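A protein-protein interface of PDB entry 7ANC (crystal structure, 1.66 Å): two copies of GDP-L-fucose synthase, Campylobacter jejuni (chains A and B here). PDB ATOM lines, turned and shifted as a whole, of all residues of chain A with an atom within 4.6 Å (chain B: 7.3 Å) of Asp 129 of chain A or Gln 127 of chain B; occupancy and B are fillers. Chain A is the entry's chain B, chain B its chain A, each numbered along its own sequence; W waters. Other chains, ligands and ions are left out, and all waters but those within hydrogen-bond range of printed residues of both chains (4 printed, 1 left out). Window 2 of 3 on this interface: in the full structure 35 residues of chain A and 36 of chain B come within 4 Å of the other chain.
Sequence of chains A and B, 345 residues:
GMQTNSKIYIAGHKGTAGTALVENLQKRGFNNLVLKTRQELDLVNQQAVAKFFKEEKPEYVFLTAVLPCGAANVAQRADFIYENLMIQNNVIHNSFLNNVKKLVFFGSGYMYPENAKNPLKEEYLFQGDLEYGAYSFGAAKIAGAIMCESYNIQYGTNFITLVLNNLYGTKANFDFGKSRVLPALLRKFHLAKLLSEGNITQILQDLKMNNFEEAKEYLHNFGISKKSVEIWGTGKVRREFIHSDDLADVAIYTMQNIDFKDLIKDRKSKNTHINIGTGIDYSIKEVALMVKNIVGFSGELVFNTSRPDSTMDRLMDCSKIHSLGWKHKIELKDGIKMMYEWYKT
Water W3 lies within hydrogen-bond range of the side-chain hydroxyl of Tyr 135 of chain A, the side-chain amide oxygen of Asn 271 of chain B and the side-chain carboxylate of Asp 129 of chain A.
Water W2 lies within hydrogen-bond range of the backbone carbonyl oxygen of Leu 130 of chain A (2.8 Å) and the side-chain amino group of Lys 270 of chain B (2.9 Å).
Water W4 lies within hydrogen-bond range of the side-chain hydroxyl of Tyr 135 of chain A (2.8 Å) and the backbone NH of Asn 271 of chain B (2.9 Å).
Water W1 lies within hydrogen-bond range of the backbone NH (N) of Asp 129 of chain A and the side-chain amide nitrogen (NE2) of Gln 127 of chain B.
Phe 126 of chain B touches its own counterpart, Phe 126 of chain A.
Phe 126 of chain A touches Gly 128 of chain B, and with the chains exchanged Gly 128 of chain A touches Phe 126 of chain B.
Phe 126 of chain A touches Asp 129 of chain B, and with the chains exchanged Asp 129 of chain A touches Phe 126 of chain B.
Positions printed for both chains: 113, 114, 126, 128 and 129.
The backbone NH of Glu 114 of chain B sits at hydrogen-bond distance from the backbone carbonyl oxygen of Asp 129 of chain B.
The backbone NH (N) of Glu 114 of chain A sits at hydrogen-bond distance from the backbone carbonyl oxygen (O) of Asp 129 of chain A (2.9 Å).
O of Leu 125 of chain B sits at hydrogen-bond distance from NE2 of Gln 127 of chain B.
Of the printed residues of chain A, Leu 125 of chain B touches Tyr 135 (3.6 Å).
Of chain A, only Asp 129 comes within 4 Å of Gln 127 of chain B.
Printed residues of chain A within 4 Å of Lys 270 of chain B: Asp 129.
The nearest printed residue of chain B that does not touch Asp 129 of chain A is Leu 125 of chain B (4.6 Å).
The backbone carbonyl oxygen (O) of Phe 126 of chain B lies within hydrogen-bond range of the backbone NH (N) of Gly 128 of chain A (2.9 Å).
The backbone carbonyl oxygen (O) of Phe 126 of chain A lies close to the backbone carbonyl oxygen (O) of Phe 126 of chain B (3.3 Å).
The backbone carbonyl oxygen of Phe 126 of chain A lies within hydrogen-bond range of the backbone NH of Gly 128 of chain B.
The side-chain carboxylate (OD2) of Asp 129 of chain A lies within salt-bridge range of the side-chain amino group (NZ) of Lys 270 of chain B.
Of the 8 printed residues of chain A, 4 touch a printed residue of chain B.
Hydrophobic or aromatic side chains of chain A that line the printed part of chain B: Phe 126 and Tyr 135.
Printed residues of chain B that touch a printed residue of chain A: Leu 125, Phe 126, Gln 127, Gly 128, Asp 129, Ile 146 and Lys 270.
Hydrophobic or aromatic side chains of chain B that line the printed part of chain A: Leu 125, Phe 126 and Ile 146.
Among the printed residues, Asp or Glu carboxylates within 4 Å of a Lys or Arg side-chain nitrogen of the other chain: Asp 129 of chain A with Lys 270 of chain B.
CD2 of Phe 126 of chain A touches OD1 of Asp 129 of chain B, at 3.5 Å.
Asp 129 of chain A touches Phe 126 of chain B (OD1 to CD2, 3.6 Å).
Asp 129 of chain A touches Gln 127 of chain B.
Tyr 135 of chain A touches Leu 125 of chain B.
Tyr 135 of chain A touches Phe 126 of chain B.
Ile 146 of chain B touches Tyr 135 of chain A.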
ATOM      1  N   PRO A 113     -22.909 -11.749 -29.080  1.00  0.00           N
ATOM      2  CA  PRO A 113     -22.822 -11.465 -27.640  1.00  0.00           C
ATOM      3  C   PRO A 113     -24.162 -11.017 -27.031  1.00  0.00           C
ATOM      4  O   PRO A 113     -24.940 -10.294 -27.708  1.00  0.00           O
ATOM      5  CB  PRO A 113     -21.798 -10.342 -27.559  1.00  0.00           C
ATOM      6  CG  PRO A 113     -20.957 -10.499 -28.789  1.00  0.00           C
ATOM      7  CD  PRO A 113     -21.928 -10.956 -29.850  1.00  0.00           C
ATOM      8  N   GLU A 114     -24.433 -11.466 -25.795  1.00  0.00           N
ATOM      9  CA  GLU A 114     -25.671 -11.119 -25.101  1.00  0.00           C
ATOM     10  C   GLU A 114     -25.853  -9.578 -25.011  1.00  0.00           C
ATOM     11  O   GLU A 114     -26.938  -9.061 -25.227  1.00  0.00           O
ATOM     12  CB  GLU A 114     -25.702 -11.701 -23.672  1.00  0.00           C
ATOM     13  CG  GLU A 114     -27.019 -11.359 -22.954  1.00  0.00           C
ATOM     14  CD  GLU A 114     -27.147 -12.017 -21.580  1.00  0.00           C
ATOM     15  OE1 GLU A 114     -26.230 -12.722 -21.185  1.00  0.00           O
ATOM     16  OE2 GLU A 114     -28.183 -11.787 -20.906  1.00  0.00           O
ATOM     17  N   PHE A 126     -17.766 -12.419 -31.650  1.00  0.00           N
ATOM     18  CA  PHE A 126     -16.679 -12.473 -30.646  1.00  0.00           C
ATOM     19  C   PHE A 126     -16.489 -11.186 -29.788  1.00  0.00           C
ATOM     20  O   PHE A 126     -15.517 -11.092 -29.032  1.00  0.00           O
ATOM     21  CB  PHE A 126     -15.304 -12.859 -31.269  1.00  0.00           C
ATOM     22  CG  PHE A 126     -15.155 -14.330 -31.682  1.00  0.00           C
ATOM     23  CD1 PHE A 126     -15.592 -15.373 -30.887  1.00  0.00           C
ATOM     24  CD2 PHE A 126     -14.516 -14.660 -32.857  1.00  0.00           C
ATOM     25  CE1 PHE A 126     -15.415 -16.713 -31.262  1.00  0.00           C
ATOM     26  CE2 PHE A 126     -14.325 -15.991 -33.233  1.00  0.00           C
ATOM     27  CZ  PHE A 126     -14.750 -17.014 -32.427  1.00  0.00           C
ATOM     28  N   GLY A 128     -17.784 -10.221 -26.921  1.00  0.00           N
ATOM     29  CA  GLY A 128     -18.372 -10.452 -25.623  1.00  0.00           C
ATOM     30  C   GLY A 128     -19.011 -11.805 -25.467  1.00  0.00           C
ATOM     31  O   GLY A 128     -19.204 -12.551 -26.446  1.00  0.00           O
ATOM     32  N   ASP A 129     -19.374 -12.105 -24.218  1.00  0.00           N
ATOM     33  CA  ASP A 129     -19.932 -13.411 -23.867  1.00  0.00           C
ATOM     34  C   ASP A 129     -21.322 -13.654 -24.447  1.00  0.00           C
ATOM     35  O   ASP A 129     -22.081 -12.716 -24.658  1.00  0.00           O
ATOM     36  CB  ASP A 129     -19.961 -13.576 -22.342  1.00  0.00           C
ATOM     37  CG  ASP A 129     -19.409 -14.909 -21.900  1.00  0.00           C
ATOM     38  OD1 ASP A 129     -19.528 -15.905 -22.666  1.00  0.00           O
ATOM     39  OD2 ASP A 129     -18.865 -14.946 -20.776  1.00  0.00           O
ATOM     40  N   LEU A 130     -21.645 -14.929 -24.723  1.00  0.00           N
ATOM     41  CA  LEU A 130     -22.943 -15.371 -25.214  1.00  0.00           C
ATOM     42  C   LEU A 130     -23.933 -15.499 -24.046  1.00  0.00           C
ATOM     43  O   LEU A 130     -23.494 -15.639 -22.882  1.00  0.00           O
ATOM     44  CB  LEU A 130     -22.806 -16.750 -25.904  1.00  0.00           C
ATOM     45  CG  LEU A 130     -21.790 -16.803 -27.060  1.00  0.00           C
ATOM     46  CD1 LEU A 130     -21.854 -18.196 -27.675  1.00  0.00           C
ATOM     47  CD2 LEU A 130     -22.013 -15.713 -28.124  1.00  0.00           C
ATOM     48  N   GLU A 131     -25.229 -15.479 -24.359  1.00  0.00           N
ATOM     49  CA  GLU A 131     -26.325 -15.717 -23.350  1.00  0.00           C
ATOM     50  C   GLU A 131     -26.166 -17.124 -22.725  1.00  0.00           C
ATOM     51  O   GLU A 131     -25.850 -18.082 -23.421  1.00  0.00           O
ATOM     52  CB  GLU A 131     -27.697 -15.556 -23.983  1.00  0.00           C
ATOM     53  CG  GLU A 131     -28.872 -15.483 -22.981  1.00  0.00           C
ATOM     54  CD  GLU A 131     -29.425 -16.865 -22.594  1.00  0.00           C
ATOM     55  OE1 GLU A 131     -29.484 -17.748 -23.502  1.00  0.00           O
ATOM     56  OE2 GLU A 131     -29.786 -17.098 -21.385  1.00  0.00           O
ATOM     57  N   TYR A 135     -25.551 -20.793 -24.627  1.00  0.00           N
ATOM     58  CA  TYR A 135     -24.091 -20.709 -24.756  1.00  0.00           C
ATOM     59  C   TYR A 135     -23.476 -21.818 -25.654  1.00  0.00           C
ATOM     60  O   TYR A 135     -22.632 -21.542 -26.515  1.00  0.00           O
ATOM     61  CB  TYR A 135     -23.498 -20.817 -23.332  1.00  0.00           C
ATOM     62  CG  TYR A 135     -21.988 -20.691 -23.154  1.00  0.00           C
ATOM     63  CD1 TYR A 135     -21.364 -19.451 -23.167  1.00  0.00           C
ATOM     64  CD2 TYR A 135     -21.194 -21.814 -22.875  1.00  0.00           C
ATOM     65  CE1 TYR A 135     -19.984 -19.340 -22.932  1.00  0.00           C
ATOM     66  CE2 TYR A 135     -19.819 -21.705 -22.634  1.00  0.00           C
ATOM     67  CZ  TYR A 135     -19.219 -20.464 -22.684  1.00  0.00           C
ATOM     68  OH  TYR A 135     -17.859 -20.337 -22.435  1.00  0.00           O
ATOM     69  N   MET B 111      -6.863 -19.531 -28.075  1.00  0.00           N
ATOM     70  CA  MET B 111      -8.312 -19.435 -27.799  1.00  0.00           C
ATOM     71  C   MET B 111      -8.719 -18.115 -27.164  1.00  0.00           C
ATOM     72  O   MET B 111      -9.930 -17.840 -27.069  1.00  0.00           O
ATOM     73  CB  MET B 111      -8.799 -20.575 -26.875  1.00  0.00           C
ATOM     74  CG  MET B 111      -8.543 -20.293 -25.381  1.00  0.00           C
ATOM     75  SD  MET B 111      -9.009 -21.595 -24.140  1.00  0.00           S
ATOM     76  CE  MET B 111      -8.679 -22.888 -25.283  1.00  0.00           C
ATOM     77  N   TYR B 112      -7.747 -17.309 -26.695  1.00  0.00           N
ATOM     78  CA  TYR B 112      -8.049 -16.023 -26.051  1.00  0.00           C
ATOM     79  C   TYR B 112      -7.948 -14.855 -27.031  1.00  0.00           C
ATOM     80  O   TYR B 112      -7.197 -14.929 -28.019  1.00  0.00           O
ATOM     81  CB  TYR B 112      -7.129 -15.797 -24.836  1.00  0.00           C
ATOM     82  CG  TYR B 112      -7.341 -16.726 -23.672  1.00  0.00           C
ATOM     83  CD1 TYR B 112      -8.550 -16.710 -22.947  1.00  0.00           C
ATOM     84  CD2 TYR B 112      -6.337 -17.598 -23.243  1.00  0.00           C
ATOM     85  CE1 TYR B 112      -8.751 -17.577 -21.884  1.00  0.00           C
ATOM     86  CE2 TYR B 112      -6.511 -18.433 -22.140  1.00  0.00           C
ATOM     87  CZ  TYR B 112      -7.731 -18.400 -21.470  1.00  0.00           C
ATOM     88  OH  TYR B 112      -7.947 -19.226 -20.411  1.00  0.00           O
ATOM     89  N   PRO B 113      -8.676 -13.732 -26.782  1.00  0.00           N
ATOM     90  CA  PRO B 113      -8.659 -12.581 -27.695  1.00  0.00           C
ATOM     91  C   PRO B 113      -7.236 -12.048 -27.980  1.00  0.00           C
ATOM     92  O   PRO B 113      -6.390 -12.031 -27.072  1.00  0.00           O
ATOM     93  CB  PRO B 113      -9.484 -11.534 -26.959  1.00  0.00           C
ATOM     94  CG  PRO B 113     -10.381 -12.349 -26.036  1.00  0.00           C
ATOM     95  CD  PRO B 113      -9.562 -13.526 -25.617  1.00  0.00           C
ATOM     96  N   GLU B 114      -6.994 -11.636 -29.229  1.00  0.00           N
ATOM     97  CA  GLU B 114      -5.677 -11.072 -29.631  1.00  0.00           C
ATOM     98  C   GLU B 114      -5.301  -9.873 -28.719  1.00  0.00           C
ATOM     99  O   GLU B 114      -4.160  -9.728 -28.312  1.00  0.00           O
ATOM    100  CB  GLU B 114      -5.717 -10.563 -31.089  1.00  0.00           C
ATOM    101  CG  GLU B 114      -4.362  -9.995 -31.515  1.00  0.00           C
ATOM    102  CD  GLU B 114      -4.275  -9.629 -32.995  1.00  0.00           C
ATOM    103  OE1 GLU B 114      -5.257  -9.785 -33.725  1.00  0.00           O
ATOM    104  OE2 GLU B 114      -3.193  -9.218 -33.419  1.00  0.00           O
ATOM    105  N   ASN B 115      -6.284  -9.023 -28.417  1.00  0.00           N
ATOM    106  CA  ASN B 115      -6.034  -7.805 -27.621  1.00  0.00           C
ATOM    107  C   ASN B 115      -6.296  -7.906 -26.104  1.00  0.00           C
ATOM    108  O   ASN B 115      -6.292  -6.904 -25.410  1.00  0.00           O
ATOM    109  CB  ASN B 115      -6.797  -6.615 -28.240  1.00  0.00           C
ATOM    110  CG  ASN B 115      -6.226  -6.197 -29.599  1.00  0.00           C
ATOM    111  OD1 ASN B 115      -5.058  -6.449 -29.902  1.00  0.00           O
ATOM    112  ND2 ASN B 115      -7.046  -5.552 -30.415  1.00  0.00           N
ATOM    113  N   ALA B 116      -6.508  -9.119 -25.588  1.00  0.00           N
ATOM    114  CA  ALA B 116      -6.708  -9.301 -24.158  1.00  0.00           C
ATOM    115  C   ALA B 116      -5.461  -8.860 -23.353  1.00  0.00           C
ATOM    116  O   ALA B 116      -4.325  -9.013 -23.796  1.00  0.00           O
ATOM    117  CB  ALA B 116      -7.018 -10.761 -23.849  1.00  0.00           C
ATOM    118  N   GLU B 122      -8.665 -16.965 -17.138  1.00  0.00           N
ATOM    119  CA  GLU B 122      -9.642 -17.870 -17.762  1.00  0.00           C
ATOM    120  C   GLU B 122     -10.925 -17.148 -18.236  1.00  0.00           C
ATOM    121  O   GLU B 122     -11.477 -17.466 -19.298  1.00  0.00           O
ATOM    122  CB  GLU B 122      -9.965 -19.052 -16.809  1.00  0.00           C
ATOM    123  CG  GLU B 122      -8.798 -20.037 -16.591  1.00  0.00           C
ATOM    124  CD  GLU B 122      -7.846 -19.669 -15.444  1.00  0.00           C
ATOM    125  OE1 GLU B 122      -7.889 -18.510 -14.878  1.00  0.00           O
ATOM    126  OE2 GLU B 122      -7.005 -20.548 -15.165  1.00  0.00           O
ATOM    127  N   GLU B 123     -11.376 -16.141 -17.465  1.00  0.00           N
ATOM    128  CA  GLU B 123     -12.552 -15.370 -17.807  1.00  0.00           C
ATOM    129  C   GLU B 123     -12.411 -14.393 -18.989  1.00  0.00           C
ATOM    130  O   GLU B 123     -13.368 -13.737 -19.352  1.00  0.00           O
ATOM    131  CB  GLU B 123     -13.138 -14.649 -16.583  1.00  0.00           C
ATOM    132  CG  GLU B 123     -12.213 -13.680 -15.912  1.00  0.00           C
ATOM    133  CD  GLU B 123     -11.450 -14.292 -14.728  1.00  0.00           C
ATOM    134  OE1 GLU B 123     -11.057 -15.533 -14.744  1.00  0.00           O
ATOM    135  OE2 GLU B 123     -11.224 -13.478 -13.768  1.00  0.00           O
ATOM    136  N   TYR B 124     -11.241 -14.334 -19.633  1.00  0.00           N
ATOM    137  CA  TYR B 124     -11.088 -13.543 -20.832  1.00  0.00           C
ATOM    138  C   TYR B 124     -11.636 -14.228 -22.111  1.00  0.00           C
ATOM    139  O   TYR B 124     -11.697 -13.605 -23.176  1.00  0.00           O
ATOM    140  CB  TYR B 124      -9.650 -13.066 -21.012  1.00  0.00           C
ATOM    141  CG  TYR B 124      -9.112 -12.114 -19.939  1.00  0.00           C
ATOM    142  CD1 TYR B 124      -9.941 -11.554 -18.950  1.00  0.00           C
ATOM    143  CD2 TYR B 124      -7.755 -11.785 -19.911  1.00  0.00           C
ATOM    144  CE1 TYR B 124      -9.416 -10.714 -17.956  1.00  0.00           C
ATOM    145  CE2 TYR B 124      -7.226 -10.934 -18.934  1.00  0.00           C
ATOM    146  CZ  TYR B 124      -8.059 -10.410 -17.952  1.00  0.00           C
ATOM    147  OH  TYR B 124      -7.504  -9.541 -17.016  1.00  0.00           O
ATOM    148  N   LEU B 125     -12.018 -15.499 -22.011  1.00  0.00           N
ATOM    149  CA  LEU B 125     -12.703 -16.203 -23.123  1.00  0.00           C
ATOM    150  C   LEU B 125     -13.889 -15.358 -23.646  1.00  0.00           C
ATOM    151  O   LEU B 125     -14.726 -14.864 -22.859  1.00  0.00           O
ATOM    152  CB  LEU B 125     -13.171 -17.583 -22.658  1.00  0.00           C
ATOM    153  CG  LEU B 125     -14.061 -18.425 -23.591  1.00  0.00           C
ATOM    154  CD1 LEU B 125     -13.333 -18.631 -24.901  1.00  0.00           C
ATOM    155  CD2 LEU B 125     -14.391 -19.782 -22.965  1.00  0.00           C
ATOM    156  N   PHE B 126     -13.945 -15.190 -24.963  1.00  0.00           N
ATOM    157  CA  PHE B 126     -14.979 -14.431 -25.681  1.00  0.00           C
ATOM    158  C   PHE B 126     -14.946 -12.891 -25.512  1.00  0.00           C
ATOM    159  O   PHE B 126     -15.841 -12.207 -25.986  1.00  0.00           O
ATOM    160  CB  PHE B 126     -16.401 -14.945 -25.400  1.00  0.00           C
ATOM    161  CG  PHE B 126     -16.761 -16.302 -26.059  1.00  0.00           C
ATOM    162  CD1 PHE B 126     -16.414 -16.614 -27.366  1.00  0.00           C
ATOM    163  CD2 PHE B 126     -17.534 -17.210 -25.373  1.00  0.00           C
ATOM    164  CE1 PHE B 126     -16.802 -17.839 -27.951  1.00  0.00           C
ATOM    165  CE2 PHE B 126     -17.959 -18.404 -25.962  1.00  0.00           C
ATOM    166  CZ  PHE B 126     -17.617 -18.696 -27.271  1.00  0.00           C
ATOM    167  N   GLN B 127     -13.891 -12.338 -24.915  1.00  0.00           N
ATOM    168  CA  GLN B 127     -13.792 -10.867 -24.723  1.00  0.00           C
ATOM    169  C   GLN B 127     -13.004 -10.183 -25.853  1.00  0.00           C
ATOM    170  O   GLN B 127     -12.062  -9.402 -25.618  1.00  0.00           O
ATOM    171  CB  GLN B 127     -13.216 -10.568 -23.319  1.00  0.00           C
ATOM    172  CG  GLN B 127     -13.974 -11.281 -22.193  1.00  0.00           C
ATOM    173  CD  GLN B 127     -15.461 -10.910 -22.124  1.00  0.00           C
ATOM    174  OE1 GLN B 127     -15.832  -9.773 -22.290  1.00  0.00           O
ATOM    175  NE2 GLN B 127     -16.307 -11.906 -21.919  1.00  0.00           N
ATOM    176  N   GLY B 128     -13.407 -10.450 -27.104  1.00  0.00           N
ATOM    177  CA  GLY B 128     -12.745  -9.894 -28.278  1.00  0.00           C
ATOM    178  C   GLY B 128     -12.327 -10.923 -29.305  1.00  0.00           C
ATOM    179  O   GLY B 128     -12.337 -12.135 -29.056  1.00  0.00           O
ATOM    180  N   ASP B 129     -11.972 -10.423 -30.491  1.00  0.00           N
ATOM    181  CA  ASP B 129     -11.679 -11.260 -31.649  1.00  0.00           C
ATOM    182  C   ASP B 129     -10.325 -11.967 -31.492  1.00  0.00           C
ATOM    183  O   ASP B 129      -9.439 -11.515 -30.745  1.00  0.00           O
ATOM    184  CB  ASP B 129     -11.675 -10.348 -32.864  1.00  0.00           C
ATOM    185  CG  ASP B 129     -12.065 -11.039 -34.151  1.00  0.00           C
ATOM    186  OD1 ASP B 129     -12.295 -12.257 -34.183  1.00  0.00           O
ATOM    187  OD2 ASP B 129     -12.040 -10.314 -35.167  1.00  0.00           O
ATOM    188  N   ILE B 146     -15.637 -25.880 -24.387  1.00  0.00           N
ATOM    189  CA  ILE B 146     -17.084 -25.800 -24.143  1.00  0.00           C
ATOM    190  C   ILE B 146     -17.761 -27.213 -24.188  1.00  0.00           C
ATOM    191  O   ILE B 146     -18.689 -27.507 -23.383  1.00  0.00           O
ATOM    192  CB  ILE B 146     -17.762 -24.720 -25.060  1.00  0.00           C
ATOM    193  CG1 ILE B 146     -17.252 -23.323 -24.716  1.00  0.00           C
ATOM    194  CG2 ILE B 146     -19.287 -24.813 -24.969  1.00  0.00           C
ATOM    195  CD1 ILE B 146     -17.730 -22.203 -25.629  1.00  0.00           C
ATOM    196  N   LYS B 270     -19.332 -21.576 -15.501  1.00  0.00           N
ATOM    197  CA  LYS B 270     -18.820 -21.076 -16.768  1.00  0.00           C
ATOM    198  C   LYS B 270     -17.315 -20.834 -16.577  1.00  0.00           C
ATOM    199  O   LYS B 270     -16.886 -20.579 -15.455  1.00  0.00           O
ATOM    200  CB  LYS B 270     -19.578 -19.798 -17.158  1.00  0.00           C
ATOM    201  CG  LYS B 270     -19.312 -19.323 -18.563  1.00  0.00           C
ATOM    202  CD  LYS B 270     -20.237 -18.175 -18.975  1.00  0.00           C
ATOM    203  CE  LYS B 270     -19.875 -16.882 -18.269  1.00  0.00           C
ATOM    204  NZ  LYS B 270     -20.799 -15.779 -18.655  1.00  0.00           N
ATOM    205  N   ASN B 271     -16.535 -20.902 -17.679  1.00  0.00           N
ATOM    206  CA  ASN B 271     -15.084 -20.691 -17.656  1.00  0.00           C
ATOM    207  C   ASN B 271     -14.393 -21.637 -16.660  1.00  0.00           C
ATOM    208  O   ASN B 271     -13.558 -21.215 -15.867  1.00  0.00           O
ATOM    209  CB  ASN B 271     -14.748 -19.210 -17.366  1.00  0.00           C
ATOM    210  CG  ASN B 271     -15.275 -18.287 -18.434  1.00  0.00           C
ATOM    211  OD1 ASN B 271     -15.160 -18.580 -19.622  1.00  0.00           O
ATOM    212  ND2 ASN B 271     -15.838 -17.149 -18.014  1.00  0.00           N
HETATM  213  O   HOH W   1     -18.861 -10.316 -22.047  1.00  0.00           O
HETATM  214  O   HOH W   2     -22.925 -16.744 -20.412  1.00  0.00           O
HETATM  215  O   HOH W   3     -17.075 -17.932 -21.548  1.00  0.00           O
HETATM  216  O   HOH W   4     -17.124 -22.038 -20.324  1.00  0.00           O
